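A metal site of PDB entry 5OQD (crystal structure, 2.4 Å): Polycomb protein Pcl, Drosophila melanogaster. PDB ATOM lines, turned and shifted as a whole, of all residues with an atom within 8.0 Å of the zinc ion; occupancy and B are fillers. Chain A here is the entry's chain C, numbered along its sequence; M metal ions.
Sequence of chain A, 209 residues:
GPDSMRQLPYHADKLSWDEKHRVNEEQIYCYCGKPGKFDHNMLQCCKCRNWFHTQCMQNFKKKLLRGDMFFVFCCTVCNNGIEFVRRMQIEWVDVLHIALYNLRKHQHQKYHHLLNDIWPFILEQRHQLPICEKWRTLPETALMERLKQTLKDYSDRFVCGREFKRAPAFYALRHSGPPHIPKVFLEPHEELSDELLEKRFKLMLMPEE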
ATOM      1  N   TYR A  29      -7.742  36.650  -0.546  1.00  0.00           N
ATOM      2  CA  TYR A  29      -7.687  35.510   0.361  1.00  0.00           C
ATOM      3  C   TYR A  29      -8.067  34.221  -0.356  1.00  0.00           C
ATOM      4  O   TYR A  29      -8.660  34.254  -1.432  1.00  0.00           O
ATOM      5  CB  TYR A  29      -8.620  35.718   1.556  1.00  0.00           C
ATOM      6  CG  TYR A  29      -8.127  36.707   2.596  1.00  0.00           C
ATOM      7  CD1 TYR A  29      -6.946  37.414   2.406  1.00  0.00           C
ATOM      8  CD2 TYR A  29      -8.832  36.920   3.769  1.00  0.00           C
ATOM      9  CE1 TYR A  29      -6.485  38.316   3.348  1.00  0.00           C
ATOM     10  CE2 TYR A  29      -8.383  37.816   4.721  1.00  0.00           C
ATOM     11  CZ  TYR A  29      -7.214  38.515   4.501  1.00  0.00           C
ATOM     12  OH  TYR A  29      -6.765  39.410   5.454  1.00  0.00           O
ATOM     13  N   CYS A  30      -7.702  33.092   0.239  1.00  0.00           N
ATOM     14  CA  CYS A  30      -8.073  31.793  -0.308  1.00  0.00           C
ATOM     15  C   CYS A  30      -9.457  31.389   0.200  1.00  0.00           C
ATOM     16  O   CYS A  30     -10.068  32.118   0.983  1.00  0.00           O
ATOM     17  CB  CYS A  30      -7.034  30.733   0.071  1.00  0.00           C
ATOM     18  SG  CYS A  30      -7.353  29.100  -0.631  1.00  0.00           S
ATOM     19  N   TYR A  31      -9.954  30.246  -0.248  1.00  0.00           N
ATOM     20  CA  TYR A  31     -11.260  29.780   0.179  1.00  0.00           C
ATOM     21  C   TYR A  31     -11.193  29.191   1.588  1.00  0.00           C
ATOM     22  O   TYR A  31     -12.220  28.938   2.210  1.00  0.00           O
ATOM     23  CB  TYR A  31     -11.826  28.748  -0.810  1.00  0.00           C
ATOM     24  CG  TYR A  31     -11.194  27.370  -0.724  1.00  0.00           C
ATOM     25  CD1 TYR A  31     -10.056  27.069  -1.458  1.00  0.00           C
ATOM     26  CD2 TYR A  31     -11.743  26.375   0.066  1.00  0.00           C
ATOM     27  CE1 TYR A  31      -9.476  25.816  -1.393  1.00  0.00           C
ATOM     28  CE2 TYR A  31     -11.175  25.115   0.142  1.00  0.00           C
ATOM     29  CZ  TYR A  31     -10.040  24.846  -0.593  1.00  0.00           C
ATOM     30  OH  TYR A  31      -9.470  23.596  -0.528  1.00  0.00           O
ATOM     31  N   CYS A  32      -9.975  28.985   2.072  1.00  0.00           N
ATOM     32  CA  CYS A  32      -9.758  28.461   3.409  1.00  0.00           C
ATOM     33  C   CYS A  32     -10.017  29.531   4.464  1.00  0.00           C
ATOM     34  O   CYS A  32     -10.324  29.225   5.621  1.00  0.00           O
ATOM     35  CB  CYS A  32      -8.335  27.920   3.556  1.00  0.00           C
ATOM     36  SG  CYS A  32      -7.046  29.156   3.316  1.00  0.00           S
ATOM     37  N   GLY A  33      -9.896  30.792   4.063  1.00  0.00           N
ATOM     38  CA  GLY A  33     -10.103  31.908   4.968  1.00  0.00           C
ATOM     39  C   GLY A  33      -8.811  32.427   5.559  1.00  0.00           C
ATOM     40  O   GLY A  33      -8.777  33.480   6.183  1.00  0.00           O
ATOM     41  N   LYS A  34      -7.731  31.665   5.353  1.00  0.00           N
ATOM     42  CA  LYS A  34      -6.420  32.054   5.856  1.00  0.00           C
ATOM     43  C   LYS A  34      -5.649  32.867   4.827  1.00  0.00           C
ATOM     44  O   LYS A  34      -5.652  32.538   3.642  1.00  0.00           O
ATOM     45  CB  LYS A  34      -5.610  30.813   6.249  1.00  0.00           C
ATOM     46  N   PRO A  35      -4.991  33.949   5.275  1.00  0.00           N
ATOM     47  CA  PRO A  35      -4.232  34.840   4.395  1.00  0.00           C
ATOM     48  C   PRO A  35      -2.940  34.196   3.885  1.00  0.00           C
ATOM     49  O   PRO A  35      -2.496  33.181   4.427  1.00  0.00           O
ATOM     50  CB  PRO A  35      -3.925  36.037   5.284  1.00  0.00           C
ATOM     51  CG  PRO A  35      -3.892  35.476   6.663  1.00  0.00           C
ATOM     52  CD  PRO A  35      -4.939  34.394   6.678  1.00  0.00           C
ATOM     53  N   GLY A  36      -2.359  34.777   2.841  1.00  0.00           N
ATOM     54  CA  GLY A  36      -1.127  34.270   2.269  1.00  0.00           C
ATOM     55  C   GLY A  36      -0.465  35.266   1.338  1.00  0.00           C
ATOM     56  O   GLY A  36      -1.050  36.288   0.997  1.00  0.00           O
ATOM     57  N   ASN A  41       3.699  30.344  -2.948  1.00  0.00           N
ATOM     58  CA  ASN A  41       2.775  29.220  -3.003  1.00  0.00           C
ATOM     59  C   ASN A  41       1.292  29.557  -3.237  1.00  0.00           C
ATOM     60  O   ASN A  41       0.425  29.029  -2.552  1.00  0.00           O
ATOM     61  CB  ASN A  41       2.921  28.362  -1.751  1.00  0.00           C
ATOM     62  CG  ASN A  41       4.325  27.827  -1.564  1.00  0.00           C
ATOM     63  OD1 ASN A  41       4.914  27.989  -0.501  1.00  0.00           O
ATOM     64  ND2 ASN A  41       4.863  27.183  -2.588  1.00  0.00           N
ATOM     65  N   MET A  42       1.001  30.446  -4.179  1.00  0.00           N
ATOM     66  CA  MET A  42      -0.379  30.787  -4.493  1.00  0.00           C
ATOM     67  C   MET A  42      -0.583  30.903  -6.004  1.00  0.00           C
ATOM     68  O   MET A  42       0.228  31.496  -6.700  1.00  0.00           O
ATOM     69  CB  MET A  42      -0.785  32.103  -3.811  1.00  0.00           C
ATOM     70  CG  MET A  42      -0.838  32.030  -2.299  1.00  0.00           C
ATOM     71  SD  MET A  42      -1.696  33.436  -1.564  1.00  0.00           S
ATOM     72  CE  MET A  42      -3.393  33.071  -1.995  1.00  0.00           C
ATOM     73  N   TRP A  51      -7.646  33.550  -5.719  1.00  0.00           N
ATOM     74  CA  TRP A  51      -6.323  33.016  -5.391  1.00  0.00           C
ATOM     75  C   TRP A  51      -6.431  31.803  -4.461  1.00  0.00           C
ATOM     76  O   TRP A  51      -7.175  31.817  -3.486  1.00  0.00           O
ATOM     77  CB  TRP A  51      -5.458  34.103  -4.755  1.00  0.00           C
ATOM     78  CG  TRP A  51      -5.183  35.245  -5.685  1.00  0.00           C
ATOM     79  CD1 TRP A  51      -5.942  36.354  -5.877  1.00  0.00           C
ATOM     80  CD2 TRP A  51      -4.053  35.375  -6.566  1.00  0.00           C
ATOM     81  NE1 TRP A  51      -5.364  37.174  -6.814  1.00  0.00           N
ATOM     82  CE2 TRP A  51      -4.210  36.596  -7.254  1.00  0.00           C
ATOM     83  CE3 TRP A  51      -2.940  34.584  -6.833  1.00  0.00           C
ATOM     84  CZ2 TRP A  51      -3.282  37.043  -8.189  1.00  0.00           C
ATOM     85  CZ3 TRP A  51      -2.014  35.021  -7.767  1.00  0.00           C
ATOM     86  CH2 TRP A  51      -2.190  36.247  -8.435  1.00  0.00           C
ATOM     87  N   PHE A  52      -5.656  30.764  -4.781  1.00  0.00           N
ATOM     88  CA  PHE A  52      -5.702  29.512  -4.041  1.00  0.00           C
ATOM     89  C   PHE A  52      -4.320  29.132  -3.506  1.00  0.00           C
ATOM     90  O   PHE A  52      -3.311  29.358  -4.168  1.00  0.00           O
ATOM     91  CB  PHE A  52      -6.239  28.381  -4.929  1.00  0.00           C
ATOM     92  CG  PHE A  52      -7.686  28.533  -5.290  1.00  0.00           C
ATOM     93  CD1 PHE A  52      -8.091  29.418  -6.271  1.00  0.00           C
ATOM     94  CD2 PHE A  52      -8.652  27.771  -4.651  1.00  0.00           C
ATOM     95  CE1 PHE A  52      -9.419  29.551  -6.613  1.00  0.00           C
ATOM     96  CE2 PHE A  52      -9.982  27.895  -4.982  1.00  0.00           C
ATOM     97  CZ  PHE A  52     -10.366  28.784  -5.963  1.00  0.00           C
ATOM     98  N   HIS A  53      -4.293  28.549  -2.307  1.00  0.00           N
ATOM     99  CA  HIS A  53      -3.054  28.009  -1.768  1.00  0.00           C
ATOM    100  C   HIS A  53      -2.682  26.721  -2.501  1.00  0.00           C
ATOM    101  O   HIS A  53      -3.542  26.076  -3.104  1.00  0.00           O
ATOM    102  CB  HIS A  53      -3.191  27.719  -0.272  1.00  0.00           C
ATOM    103  CG  HIS A  53      -3.268  28.947   0.579  1.00  0.00           C
ATOM    104  ND1 HIS A  53      -4.417  29.332   1.232  1.00  0.00           N
ATOM    105  CD2 HIS A  53      -2.329  29.876   0.897  1.00  0.00           C
ATOM    106  CE1 HIS A  53      -4.192  30.452   1.903  1.00  0.00           C
ATOM    107  NE2 HIS A  53      -2.924  30.798   1.718  1.00  0.00           N
ATOM    108  N   THR A  54      -1.411  26.360  -2.466  1.00  0.00           N
ATOM    109  CA  THR A  54      -0.958  25.106  -3.060  1.00  0.00           C
ATOM    110  C   THR A  54      -1.384  23.939  -2.188  1.00  0.00           C
ATOM    111  O   THR A  54      -1.537  22.815  -2.659  1.00  0.00           O
ATOM    112  CB  THR A  54       0.569  25.080  -3.241  1.00  0.00           C
ATOM    113  OG1 THR A  54       1.208  25.317  -1.980  1.00  0.00           O
ATOM    114  CG2 THR A  54       1.016  26.127  -4.241  1.00  0.00           C
ATOM    115  N   GLN A  55      -1.589  24.217  -0.900  1.00  0.00           N
ATOM    116  CA  GLN A  55      -2.058  23.206   0.039  1.00  0.00           C
ATOM    117  C   GLN A  55      -3.577  23.060  -0.046  1.00  0.00           C
ATOM    118  O   GLN A  55      -4.104  21.955   0.025  1.00  0.00           O
ATOM    119  CB  GLN A  55      -1.651  23.584   1.470  1.00  0.00           C
ATOM    120  CG  GLN A  55      -0.177  23.927   1.633  1.00  0.00           C
ATOM    121  CD  GLN A  55       0.137  24.431   3.023  1.00  0.00           C
ATOM    122  OE1 GLN A  55      -0.720  24.450   3.900  1.00  0.00           O
ATOM    123  NE2 GLN A  55       1.386  24.861   3.227  1.00  0.00           N
ATOM    124  N   CYS A  56      -4.258  24.192  -0.199  1.00  0.00           N
ATOM    125  CA  CYS A  56      -5.716  24.208  -0.237  1.00  0.00           C
ATOM    126  C   CYS A  56      -6.250  23.605  -1.534  1.00  0.00           C
ATOM    127  O   CYS A  56      -7.395  23.173  -1.608  1.00  0.00           O
ATOM    128  CB  CYS A  56      -6.232  25.634  -0.066  1.00  0.00           C
ATOM    129  SG  CYS A  56      -5.898  26.343   1.561  1.00  0.00           S
ATOM    130  N   MET A  57      -5.374  23.497  -2.529  1.00  0.00           N
ATOM    131  CA  MET A  57      -5.721  22.859  -3.797  1.00  0.00           C
ATOM    132  C   MET A  57      -5.262  21.409  -3.778  1.00  0.00           C
ATOM    133  O   MET A  57      -4.115  21.124  -3.442  1.00  0.00           O
ATOM    134  CB  MET A  57      -5.099  23.613  -4.974  1.00  0.00           C
ATOM    135  CG  MET A  57      -3.578  23.560  -5.035  1.00  0.00           C
ATOM    136  SD  MET A  57      -2.885  24.104  -6.609  1.00  0.00           S
ATOM    137  CE  MET A  57      -3.705  25.680  -6.817  1.00  0.00           C
HETATM  138 ZN    ZN M   1      -6.157  28.573   1.258  1.00  0.00          ZN
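The side-chain sulfur (SG) of Cys 32 lies close to the backbone NH (N) of Lys 34 (3.3 Å).
Of the 17 residues printed, 4 come within 4 Å of the zinc ion.
The zinc ion is bound by a ring nitrogen (ND1) of His 53 (1.9 Å). SG of Cys 56 is bound to the zinc ion (2.3 Å). SG of Cys 30 binds the zinc ion (2.3 Å). SG of Cys 32 is bound to the zinc ion (2.3 Å). The zinc ion has four donor atoms within binding distance.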
